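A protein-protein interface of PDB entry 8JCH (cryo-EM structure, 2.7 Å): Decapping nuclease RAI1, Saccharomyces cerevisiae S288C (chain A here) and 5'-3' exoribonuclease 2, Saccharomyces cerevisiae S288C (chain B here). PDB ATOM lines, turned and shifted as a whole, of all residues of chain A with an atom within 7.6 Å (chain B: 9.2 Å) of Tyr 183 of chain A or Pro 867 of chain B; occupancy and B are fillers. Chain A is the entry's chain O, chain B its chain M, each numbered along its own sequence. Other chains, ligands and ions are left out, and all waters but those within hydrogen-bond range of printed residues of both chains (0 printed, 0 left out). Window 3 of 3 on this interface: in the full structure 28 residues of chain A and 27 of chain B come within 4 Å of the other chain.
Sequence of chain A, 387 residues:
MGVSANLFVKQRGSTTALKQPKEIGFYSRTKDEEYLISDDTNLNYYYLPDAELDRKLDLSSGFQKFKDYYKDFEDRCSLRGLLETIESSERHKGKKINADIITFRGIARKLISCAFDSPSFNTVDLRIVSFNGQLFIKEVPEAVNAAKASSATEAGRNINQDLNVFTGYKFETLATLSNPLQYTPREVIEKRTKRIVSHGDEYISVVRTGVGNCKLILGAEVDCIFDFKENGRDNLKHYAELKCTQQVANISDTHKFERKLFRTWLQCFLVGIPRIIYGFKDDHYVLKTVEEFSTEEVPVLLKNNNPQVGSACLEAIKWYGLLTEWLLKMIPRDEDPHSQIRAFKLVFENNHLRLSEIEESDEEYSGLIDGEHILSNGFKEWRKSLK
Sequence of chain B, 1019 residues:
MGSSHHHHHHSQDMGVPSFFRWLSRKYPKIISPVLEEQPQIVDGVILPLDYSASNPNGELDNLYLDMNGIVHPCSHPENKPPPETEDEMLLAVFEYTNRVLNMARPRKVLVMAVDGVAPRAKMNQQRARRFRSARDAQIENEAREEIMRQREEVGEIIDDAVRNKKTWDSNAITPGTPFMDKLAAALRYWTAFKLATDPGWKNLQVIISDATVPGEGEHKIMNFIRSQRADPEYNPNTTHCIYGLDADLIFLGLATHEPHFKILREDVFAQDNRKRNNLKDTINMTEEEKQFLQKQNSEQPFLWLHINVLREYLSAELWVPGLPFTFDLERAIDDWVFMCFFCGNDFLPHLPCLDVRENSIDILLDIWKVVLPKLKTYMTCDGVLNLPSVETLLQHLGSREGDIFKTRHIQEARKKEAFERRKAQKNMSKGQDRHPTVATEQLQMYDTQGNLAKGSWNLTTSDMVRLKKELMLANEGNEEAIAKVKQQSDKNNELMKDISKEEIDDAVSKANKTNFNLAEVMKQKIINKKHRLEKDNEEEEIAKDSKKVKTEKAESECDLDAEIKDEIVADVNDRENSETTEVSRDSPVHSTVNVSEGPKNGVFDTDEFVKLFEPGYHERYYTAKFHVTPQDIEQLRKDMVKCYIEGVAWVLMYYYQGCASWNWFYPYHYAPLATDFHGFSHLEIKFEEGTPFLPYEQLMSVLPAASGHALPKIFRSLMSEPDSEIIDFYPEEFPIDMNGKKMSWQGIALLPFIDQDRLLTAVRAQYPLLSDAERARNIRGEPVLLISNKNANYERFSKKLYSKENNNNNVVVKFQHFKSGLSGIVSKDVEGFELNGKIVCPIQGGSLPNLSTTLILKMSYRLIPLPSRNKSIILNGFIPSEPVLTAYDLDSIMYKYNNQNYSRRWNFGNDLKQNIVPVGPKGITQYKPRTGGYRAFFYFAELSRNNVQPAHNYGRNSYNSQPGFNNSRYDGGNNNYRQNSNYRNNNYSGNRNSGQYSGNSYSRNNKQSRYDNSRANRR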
ATOM      1  N   LEU A 177      26.514   8.184 -27.255  1.00  0.00           N
ATOM      2  CA  LEU A 177      25.334   8.624 -26.527  1.00  0.00           C
ATOM      3  C   LEU A 177      24.116   8.504 -27.432  1.00  0.00           C
ATOM      4  O   LEU A 177      24.183   8.765 -28.635  1.00  0.00           O
ATOM      5  CB  LEU A 177      25.489  10.067 -26.027  1.00  0.00           C
ATOM      6  CG  LEU A 177      24.435  10.580 -25.043  1.00  0.00           C
ATOM      7  CD1 LEU A 177      24.325   9.654 -23.844  1.00  0.00           C
ATOM      8  CD2 LEU A 177      24.769  11.997 -24.604  1.00  0.00           C
ATOM      9  N   ASN A 179      20.894  10.138 -27.453  1.00  0.00           N
ATOM     10  CA  ASN A 179      20.409  11.404 -27.972  1.00  0.00           C
ATOM     11  C   ASN A 179      21.510  12.456 -27.844  1.00  0.00           C
ATOM     12  O   ASN A 179      22.525  12.228 -27.182  1.00  0.00           O
ATOM     13  CB  ASN A 179      19.136  11.817 -27.231  1.00  0.00           C
ATOM     14  CG  ASN A 179      19.417  12.406 -25.865  1.00  0.00           C
ATOM     15  OD1 ASN A 179      20.301  11.942 -25.144  1.00  0.00           O
ATOM     16  ND2 ASN A 179      18.670  13.443 -25.503  1.00  0.00           N
ATOM     17  N   PRO A 180      21.353  13.616 -28.492  1.00  0.00           N
ATOM     18  CA  PRO A 180      22.377  14.663 -28.374  1.00  0.00           C
ATOM     19  C   PRO A 180      22.578  15.104 -26.931  1.00  0.00           C
ATOM     20  O   PRO A 180      21.654  15.086 -26.115  1.00  0.00           O
ATOM     21  CB  PRO A 180      21.826  15.803 -29.241  1.00  0.00           C
ATOM     22  CG  PRO A 180      20.393  15.445 -29.514  1.00  0.00           C
ATOM     23  CD  PRO A 180      20.349  13.960 -29.511  1.00  0.00           C
ATOM     24  N   LEU A 181      23.819  15.490 -26.623  1.00  0.00           N
ATOM     25  CA  LEU A 181      24.207  15.756 -25.241  1.00  0.00           C
ATOM     26  C   LEU A 181      23.424  16.925 -24.652  1.00  0.00           C
ATOM     27  O   LEU A 181      23.014  16.886 -23.487  1.00  0.00           O
ATOM     28  CB  LEU A 181      25.711  16.021 -25.162  1.00  0.00           C
ATOM     29  CG  LEU A 181      26.264  16.423 -23.794  1.00  0.00           C
ATOM     30  CD1 LEU A 181      25.952  15.361 -22.750  1.00  0.00           C
ATOM     31  CD2 LEU A 181      27.758  16.670 -23.886  1.00  0.00           C
ATOM     32  N   GLN A 182      23.215  17.979 -25.442  1.00  0.00           N
ATOM     33  CA  GLN A 182      22.521  19.169 -24.960  1.00  0.00           C
ATOM     34  C   GLN A 182      21.121  18.827 -24.466  1.00  0.00           C
ATOM     35  O   GLN A 182      20.618  19.451 -23.527  1.00  0.00           O
ATOM     36  CB  GLN A 182      22.450  20.251 -26.049  1.00  0.00           C
ATOM     37  CG  GLN A 182      23.786  20.748 -26.656  1.00  0.00           C
ATOM     38  CD  GLN A 182      24.607  19.701 -27.410  1.00  0.00           C
ATOM     39  OE1 GLN A 182      24.573  18.509 -27.106  1.00  0.00           O
ATOM     40  NE2 GLN A 182      25.358  20.162 -28.405  1.00  0.00           N
ATOM     41  N   TYR A 183      20.485  17.840 -25.094  1.00  0.00           N
ATOM     42  CA  TYR A 183      19.172  17.368 -24.681  1.00  0.00           C
ATOM     43  C   TYR A 183      19.252  16.126 -23.800  1.00  0.00           C
ATOM     44  O   TYR A 183      18.217  15.516 -23.513  1.00  0.00           O
ATOM     45  CB  TYR A 183      18.295  17.093 -25.908  1.00  0.00           C
ATOM     46  CG  TYR A 183      18.295  18.201 -26.947  1.00  0.00           C
ATOM     47  CD1 TYR A 183      19.292  18.282 -27.914  1.00  0.00           C
ATOM     48  CD2 TYR A 183      17.305  19.173 -26.950  1.00  0.00           C
ATOM     49  CE1 TYR A 183      19.292  19.292 -28.861  1.00  0.00           C
ATOM     50  CE2 TYR A 183      17.298  20.188 -27.891  1.00  0.00           C
ATOM     51  CZ  TYR A 183      18.294  20.243 -28.842  1.00  0.00           C
ATOM     52  OH  TYR A 183      18.288  21.253 -29.778  1.00  0.00           O
ATOM     53  N   THR A 184      20.454  15.740 -23.367  1.00  0.00           N
ATOM     54  CA  THR A 184      20.631  14.549 -22.550  1.00  0.00           C
ATOM     55  C   THR A 184      20.703  14.941 -21.084  1.00  0.00           C
ATOM     56  O   THR A 184      21.583  15.730 -20.707  1.00  0.00           O
ATOM     57  CB  THR A 184      21.897  13.799 -22.949  1.00  0.00           C
ATOM     58  OG1 THR A 184      21.836  13.459 -24.339  1.00  0.00           O
ATOM     59  CG2 THR A 184      22.029  12.520 -22.134  1.00  0.00           C
ATOM     60  N   PRO A 185      19.813  14.433 -20.233  1.00  0.00           N
ATOM     61  CA  PRO A 185      19.906  14.732 -18.800  1.00  0.00           C
ATOM     62  C   PRO A 185      21.171  14.152 -18.183  1.00  0.00           C
ATOM     63  O   PRO A 185      21.756  13.186 -18.679  1.00  0.00           O
ATOM     64  CB  PRO A 185      18.650  14.072 -18.217  1.00  0.00           C
ATOM     65  CG  PRO A 185      17.710  13.954 -19.377  1.00  0.00           C
ATOM     66  CD  PRO A 185      18.585  13.692 -20.564  1.00  0.00           C
ATOM     67  N   ARG A 186      21.597  14.774 -17.081  1.00  0.00           N
ATOM     68  CA  ARG A 186      22.811  14.342 -16.394  1.00  0.00           C
ATOM     69  C   ARG A 186      22.665  12.923 -15.854  1.00  0.00           C
ATOM     70  O   ARG A 186      23.616  12.131 -15.887  1.00  0.00           O
ATOM     71  CB  ARG A 186      23.144  15.318 -15.264  1.00  0.00           C
ATOM     72  CG  ARG A 186      24.356  14.927 -14.437  1.00  0.00           C
ATOM     73  CD  ARG A 186      24.620  15.935 -13.332  1.00  0.00           C
ATOM     74  NE  ARG A 186      25.009  17.239 -13.857  1.00  0.00           N
ATOM     75  CZ  ARG A 186      26.262  17.621 -14.059  1.00  0.00           C
ATOM     76  NH1 ARG A 186      27.280  16.820 -13.791  1.00  0.00           N
ATOM     77  NH2 ARG A 186      26.500  18.837 -14.540  1.00  0.00           N
ATOM     78  N   VAL A 188      20.993  10.541 -17.132  1.00  0.00           N
ATOM     79  CA  VAL A 188      21.185   9.631 -18.258  1.00  0.00           C
ATOM     80  C   VAL A 188      22.669   9.381 -18.491  1.00  0.00           C
ATOM     81  O   VAL A 188      23.090   8.249 -18.754  1.00  0.00           O
ATOM     82  CB  VAL A 188      20.494  10.183 -19.519  1.00  0.00           C
ATOM     83  CG1 VAL A 188      20.734   9.262 -20.704  1.00  0.00           C
ATOM     84  CG2 VAL A 188      19.005  10.352 -19.269  1.00  0.00           C
ATOM     85  N   ARG B 226      24.413  31.075 -21.645  1.00  0.00           N
ATOM     86  CA  ARG B 226      23.860  29.734 -21.490  1.00  0.00           C
ATOM     87  C   ARG B 226      22.962  29.364 -22.664  1.00  0.00           C
ATOM     88  O   ARG B 226      22.974  28.215 -23.122  1.00  0.00           O
ATOM     89  CB  ARG B 226      23.093  29.637 -20.175  1.00  0.00           C
ATOM     90  CG  ARG B 226      23.978  29.623 -18.940  1.00  0.00           C
ATOM     91  CD  ARG B 226      23.131  29.589 -17.686  1.00  0.00           C
ATOM     92  NE  ARG B 226      21.795  30.106 -17.954  1.00  0.00           N
ATOM     93  CZ  ARG B 226      21.111  30.886 -17.129  1.00  0.00           C
ATOM     94  NH1 ARG B 226      21.605  31.259 -15.961  1.00  0.00           N
ATOM     95  NH2 ARG B 226      19.904  31.310 -17.491  1.00  0.00           N
ATOM     96  N   SER B 227      22.169  30.319 -23.159  1.00  0.00           N
ATOM     97  CA  SER B 227      21.317  30.044 -24.313  1.00  0.00           C
ATOM     98  C   SER B 227      22.149  29.736 -25.552  1.00  0.00           C
ATOM     99  O   SER B 227      21.813  28.831 -26.326  1.00  0.00           O
ATOM    100  CB  SER B 227      20.386  31.228 -24.571  1.00  0.00           C
ATOM    101  OG  SER B 227      21.101  32.334 -25.096  1.00  0.00           O
ATOM    102  N   GLN B 228      23.236  30.482 -25.759  1.00  0.00           N
ATOM    103  CA  GLN B 228      24.105  30.228 -26.903  1.00  0.00           C
ATOM    104  C   GLN B 228      24.810  28.884 -26.774  1.00  0.00           C
ATOM    105  O   GLN B 228      25.014  28.185 -27.774  1.00  0.00           O
ATOM    106  CB  GLN B 228      25.123  31.358 -27.048  1.00  0.00           C
ATOM    107  CG  GLN B 228      25.764  31.440 -28.422  1.00  0.00           C
ATOM    108  CD  GLN B 228      24.887  32.154 -29.431  1.00  0.00           C
ATOM    109  OE1 GLN B 228      25.052  31.991 -30.639  1.00  0.00           O
ATOM    110  NE2 GLN B 228      23.945  32.950 -28.937  1.00  0.00           N
ATOM    111  N   ARG B 229      25.192  28.505 -25.552  1.00  0.00           N
ATOM    112  CA  ARG B 229      25.841  27.216 -25.342  1.00  0.00           C
ATOM    113  C   ARG B 229      24.904  26.045 -25.604  1.00  0.00           C
ATOM    114  O   ARG B 229      25.378  24.919 -25.795  1.00  0.00           O
ATOM    115  CB  ARG B 229      26.393  27.130 -23.918  1.00  0.00           C
ATOM    116  CG  ARG B 229      27.593  26.207 -23.774  1.00  0.00           C
ATOM    117  CD  ARG B 229      28.341  26.470 -22.478  1.00  0.00           C
ATOM    118  NE  ARG B 229      27.577  26.045 -21.311  1.00  0.00           N
ATOM    119  CZ  ARG B 229      27.641  24.835 -20.774  1.00  0.00           C
ATOM    120  NH1 ARG B 229      28.429  23.898 -21.274  1.00  0.00           N
ATOM    121  NH2 ARG B 229      26.895  24.557 -19.708  1.00  0.00           N
ATOM    122  N   ALA B 230      23.593  26.278 -25.621  1.00  0.00           N
ATOM    123  CA  ALA B 230      22.624  25.222 -25.881  1.00  0.00           C
ATOM    124  C   ALA B 230      22.352  25.014 -27.365  1.00  0.00           C
ATOM    125  O   ALA B 230      21.592  24.106 -27.716  1.00  0.00           O
ATOM    126  CB  ALA B 230      21.311  25.522 -25.155  1.00  0.00           C
ATOM    127  N   ASP B 231      22.944  25.826 -28.236  1.00  0.00           N
ATOM    128  CA  ASP B 231      22.724  25.663 -29.665  1.00  0.00           C
ATOM    129  C   ASP B 231      23.422  24.398 -30.163  1.00  0.00           C
ATOM    130  O   ASP B 231      24.560  24.121 -29.772  1.00  0.00           O
ATOM    131  CB  ASP B 231      23.240  26.879 -30.431  1.00  0.00           C
ATOM    132  CG  ASP B 231      23.007  26.769 -31.924  1.00  0.00           C
ATOM    133  OD1 ASP B 231      21.852  26.952 -32.363  1.00  0.00           O
ATOM    134  OD2 ASP B 231      23.978  26.497 -32.660  1.00  0.00           O
ATOM    135  N   PRO B 232      22.762  23.607 -31.012  1.00  0.00           N
ATOM    136  CA  PRO B 232      23.410  22.390 -31.531  1.00  0.00           C
ATOM    137  C   PRO B 232      24.683  22.665 -32.313  1.00  0.00           C
ATOM    138  O   PRO B 232      25.609  21.844 -32.276  1.00  0.00           O
ATOM    139  CB  PRO B 232      22.324  21.769 -32.423  1.00  0.00           C
ATOM    140  CG  PRO B 232      21.038  22.344 -31.921  1.00  0.00           C
ATOM    141  CD  PRO B 232      21.367  23.732 -31.465  1.00  0.00           C
ATOM    142  N   GLU B 233      24.762  23.793 -33.016  1.00  0.00           N
ATOM    143  CA  GLU B 233      25.918  24.133 -33.834  1.00  0.00           C
ATOM    144  C   GLU B 233      26.875  25.086 -33.127  1.00  0.00           C
ATOM    145  O   GLU B 233      27.734  25.688 -33.780  1.00  0.00           O
ATOM    146  CB  GLU B 233      25.465  24.733 -35.165  1.00  0.00           C
ATOM    147  CG  GLU B 233      24.132  24.204 -35.667  1.00  0.00           C
ATOM    148  CD  GLU B 233      24.215  22.767 -36.140  1.00  0.00           C
ATOM    149  OE1 GLU B 233      24.876  22.516 -37.169  1.00  0.00           O
ATOM    150  OE2 GLU B 233      23.617  21.888 -35.485  1.00  0.00           O
ATOM    151  N   GLN B 657      21.141  28.889 -13.177  1.00  0.00           N
ATOM    152  CA  GLN B 657      20.276  28.602 -14.323  1.00  0.00           C
ATOM    153  C   GLN B 657      18.974  29.386 -14.170  1.00  0.00           C
ATOM    154  O   GLN B 657      18.102  29.002 -13.386  1.00  0.00           O
ATOM    155  CB  GLN B 657      20.021  27.105 -14.442  1.00  0.00           C
ATOM    156  CG  GLN B 657      19.071  26.716 -15.556  1.00  0.00           C
ATOM    157  CD  GLN B 657      18.127  25.600 -15.149  1.00  0.00           C
ATOM    158  OE1 GLN B 657      18.212  25.074 -14.040  1.00  0.00           O
ATOM    159  NE2 GLN B 657      17.221  25.234 -16.047  1.00  0.00           N
ATOM    160  N   LYS B 814      14.867  30.653 -37.333  1.00  0.00           N
ATOM    161  CA  LYS B 814      15.556  29.857 -36.320  1.00  0.00           C
ATOM    162  C   LYS B 814      16.958  29.500 -36.791  1.00  0.00           C
ATOM    163  O   LYS B 814      17.401  28.352 -36.705  1.00  0.00           O
ATOM    164  CB  LYS B 814      14.761  28.599 -35.983  1.00  0.00           C
ATOM    165  CG  LYS B 814      14.788  28.225 -34.510  1.00  0.00           C
ATOM    166  CD  LYS B 814      14.226  26.832 -34.282  1.00  0.00           C
ATOM    167  CE  LYS B 814      15.310  25.773 -34.405  1.00  0.00           C
ATOM    168  NZ  LYS B 814      14.910  24.492 -33.760  1.00  0.00           N
ATOM    169  N   GLN B 816      20.841  28.983 -36.771  1.00  0.00           N
ATOM    170  CA  GLN B 816      21.703  28.479 -35.716  1.00  0.00           C
ATOM    171  C   GLN B 816      23.067  29.165 -35.773  1.00  0.00           C
ATOM    172  O   GLN B 816      23.282  30.119 -36.526  1.00  0.00           O
ATOM    173  CB  GLN B 816      21.825  26.959 -35.830  1.00  0.00           C
ATOM    174  CG  GLN B 816      20.500  26.243 -36.031  1.00  0.00           C
ATOM    175  CD  GLN B 816      19.619  26.287 -34.798  1.00  0.00           C
ATOM    176  OE1 GLN B 816      19.805  25.509 -33.862  1.00  0.00           O
ATOM    177  NE2 GLN B 816      18.655  27.199 -34.792  1.00  0.00           N
ATOM    178  N   ILE B 864      16.465  31.950 -27.486  1.00  0.00           N
ATOM    179  CA  ILE B 864      15.859  30.624 -27.641  1.00  0.00           C
ATOM    180  C   ILE B 864      15.684  29.992 -26.265  1.00  0.00           C
ATOM    181  O   ILE B 864      16.657  29.920 -25.491  1.00  0.00           O
ATOM    182  CB  ILE B 864      16.725  29.745 -28.546  1.00  0.00           C
ATOM    183  CG1 ILE B 864      16.509  30.120 -30.014  1.00  0.00           C
ATOM    184  CG2 ILE B 864      16.412  28.272 -28.322  1.00  0.00           C
ATOM    185  CD1 ILE B 864      17.216  29.204 -30.989  1.00  0.00           C
ATOM    186  N   PRO B 865      14.482  29.541 -25.905  1.00  0.00           N
ATOM    187  CA  PRO B 865      14.295  28.902 -24.596  1.00  0.00           C
ATOM    188  C   PRO B 865      15.139  27.642 -24.468  1.00  0.00           C
ATOM    189  O   PRO B 865      15.344  26.906 -25.436  1.00  0.00           O
ATOM    190  CB  PRO B 865      12.796  28.582 -24.566  1.00  0.00           C
ATOM    191  CG  PRO B 865      12.185  29.482 -25.595  1.00  0.00           C
ATOM    192  CD  PRO B 865      13.223  29.642 -26.659  1.00  0.00           C
ATOM    193  N   LEU B 866      15.630  27.403 -23.261  1.00  0.00           N
ATOM    194  CA  LEU B 866      16.469  26.238 -23.007  1.00  0.00           C
ATOM    195  C   LEU B 866      15.618  24.974 -23.005  1.00  0.00           C
ATOM    196  O   LEU B 866      14.655  24.890 -22.232  1.00  0.00           O
ATOM    197  CB  LEU B 866      17.198  26.390 -21.676  1.00  0.00           C
ATOM    198  CG  LEU B 866      18.670  26.798 -21.757  1.00  0.00           C
ATOM    199  CD1 LEU B 866      18.800  28.286 -22.046  1.00  0.00           C
ATOM    200  CD2 LEU B 866      19.399  26.433 -20.474  1.00  0.00           C
ATOM    201  N   PRO B 867      15.919  23.984 -23.849  1.00  0.00           N
ATOM    202  CA  PRO B 867      15.134  22.739 -23.825  1.00  0.00           C
ATOM    203  C   PRO B 867      15.190  22.015 -22.493  1.00  0.00           C
ATOM    204  O   PRO B 867      14.197  21.397 -22.091  1.00  0.00           O
ATOM    205  CB  PRO B 867      15.767  21.906 -24.949  1.00  0.00           C
ATOM    206  CG  PRO B 867      16.471  22.900 -25.821  1.00  0.00           C
ATOM    207  CD  PRO B 867      16.949  23.974 -24.900  1.00  0.00           C
ATOM    208  N   SER B 868      16.321  22.072 -21.795  1.00  0.00           N
ATOM    209  CA  SER B 868      16.477  21.413 -20.505  1.00  0.00           C
ATOM    210  C   SER B 868      17.336  22.306 -19.615  1.00  0.00           C
ATOM    211  O   SER B 868      17.608  23.465 -19.941  1.00  0.00           O
ATOM    212  CB  SER B 868      17.080  20.012 -20.678  1.00  0.00           C
ATOM    213  OG  SER B 868      16.345  19.253 -21.623  1.00  0.00           O
ATOM    214  N   ARG B 869      17.762  21.760 -18.481  1.00  0.00           N
ATOM    215  CA  ARG B 869      18.604  22.505 -17.557  1.00  0.00           C
ATOM    216  C   ARG B 869      19.989  22.729 -18.152  1.00  0.00           C
ATOM    217  O   ARG B 869      20.506  21.907 -18.913  1.00  0.00           O
ATOM    218  CB  ARG B 869      18.719  21.767 -16.224  1.00  0.00           C
ATOM    219  CG  ARG B 869      17.426  21.116 -15.763  1.00  0.00           C
ATOM    220  CD  ARG B 869      17.472  20.787 -14.281  1.00  0.00           C
ATOM    221  NE  ARG B 869      17.363  21.982 -13.454  1.00  0.00           N
ATOM    222  CZ  ARG B 869      17.429  21.986 -12.129  1.00  0.00           C
ATOM    223  NH1 ARG B 869      17.606  20.869 -11.444  1.00  0.00           N
ATOM    224  NH2 ARG B 869      17.314  23.139 -11.478  1.00  0.00           N
ATOM    225  N   ASN B 870      20.592  23.864 -17.795  1.00  0.00           N
ATOM    226  CA  ASN B 870      21.920  24.229 -18.288  1.00  0.00           C
ATOM    227  C   ASN B 870      22.958  23.381 -17.557  1.00  0.00           C
ATOM    228  O   ASN B 870      23.570  23.790 -16.568  1.00  0.00           O
ATOM    229  CB  ASN B 870      22.174  25.719 -18.097  1.00  0.00           C
ATOM    230  CG  ASN B 870      23.511  26.158 -18.661  1.00  0.00           C
ATOM    231  OD1 ASN B 870      23.666  26.312 -19.873  1.00  0.00           O
ATOM    232  ND2 ASN B 870      24.485  26.363 -17.783  1.00  0.00           N
ATOM    233  N   LYS B 871      23.150  22.166 -18.064  1.00  0.00           N
ATOM    234  CA  LYS B 871      24.102  21.242 -17.464  1.00  0.00           C
ATOM    235  C   LYS B 871      25.528  21.752 -17.637  1.00  0.00           C
ATOM    236  O   LYS B 871      25.917  22.204 -18.717  1.00  0.00           O
ATOM    237  CB  LYS B 871      23.955  19.855 -18.090  1.00  0.00           C
ATOM    238  CG  LYS B 871      24.902  18.810 -17.525  1.00  0.00           C
ATOM    239  CD  LYS B 871      24.509  17.408 -17.965  1.00  0.00           C
ATOM    240  CE  LYS B 871      24.172  17.360 -19.448  1.00  0.00           C
ATOM    241  NZ  LYS B 871      25.351  17.676 -20.300  1.00  0.00           N
ATOM    242  N   LEU B 875      31.626  20.979 -23.596  1.00  0.00           N
ATOM    243  CA  LEU B 875      31.159  20.554 -24.907  1.00  0.00           C
ATOM    244  C   LEU B 875      32.209  19.699 -25.607  1.00  0.00           C
ATOM    245  O   LEU B 875      33.416  19.891 -25.438  1.00  0.00           O
ATOM    246  CB  LEU B 875      30.814  21.768 -25.769  1.00  0.00           C
ATOM    247  CG  LEU B 875      29.326  22.064 -25.970  1.00  0.00           C
ATOM    248  CD1 LEU B 875      28.675  20.987 -26.824  1.00  0.00           C
ATOM    249  CD2 LEU B 875      28.616  22.193 -24.631  1.00  0.00           C
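The guanidinium group (NH2) of Arg 229 of chain B is in hydrogen-bond range of the backbone carbonyl oxygen (O) of Lys 871 of chain B, at 2.7 Å.
The backbone carbonyl oxygen (O) of Tyr 183 of chain A is in hydrogen-bond range of the side-chain amide nitrogen (ND2) of Asn 179 of chain A.
The backbone carbonyl oxygen (O) of Asn 179 of chain A lies close to the side-chain hydroxyl (OG1) of Thr 184 of chain A, 3.2 Å away.
The backbone carbonyl oxygen (O) of Pro 180 of chain A sits at hydrogen-bond distance from the side-chain hydroxyl (OG1) of Thr 184 of chain A (2.4 Å).
Among the printed residues, merely in contact across the chains: Thr 184 of chain A with Lys 871 of chain B (3.3 Å), Arg 186 of chain A with Lys 871 of chain B (3.4 Å), Leu 181 of chain A with Lys 871 of chain B (3.4 Å), Tyr 183 of chain A with Pro 867 of chain B (3.5 Å), Tyr 183 of chain A with Pro 232 of chain B (3.7 Å) and Gln 182 of chain A with Leu 875 of chain B (3.8 Å).
Tyr 183 of chain A touches just these residues of chain B: Pro 232 (3.7 Å) and Pro 867 (3.5 Å).
Of chain A, only Tyr 183 comes within 4 Å of Pro 867 of chain B.
No residue of chain B comes within 4 Å of Pro 180 of chain A.
Of chain B, only Lys 871 (3.3 Å) comes within 4 Å of Thr 184 of chain A.
Of the printed residues of chain A, Pro 232 of chain B touches Tyr 183.
Of the printed residues of chain B, Leu 181 of chain A touches Lys 871.
Printed residues of chain A within 4 Å of Lys 871 of chain B: Leu 181 (3.4 Å), Thr 184 (3.3 Å) and Arg 186 (3.4 Å).
Printed residues of chain B within 4 Å of Gln 182 of chain A: Leu 875 (3.8 Å).
Of the printed residues of chain B, Arg 186 of chain A touches Lys 871.
Arg 869 of chain B touches none of the printed residues of chain A.
Leu 866 of chain B touches none of the printed residues of chain A.
The nearest residue of chain B that does not touch Tyr 183 of chain A is Ser 868 of chain B (4.6 Å).
The nearest printed residue of chain B that does not touch Leu 181 of chain A is Leu 875 of chain B (5.3 Å).
Of the 10 printed residues of chain A, 5 touch a printed residue of chain B.
Hydrophobic or aromatic side chains of chain A that line the printed part of chain B: Leu 181 and Tyr 183.
Among the printed residues, 6 pairs touch across the chains.
Among the printed residues, no Asp or Glu carboxylate lies within 4 Å of a Lys or Arg side-chain nitrogen of the other chain.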
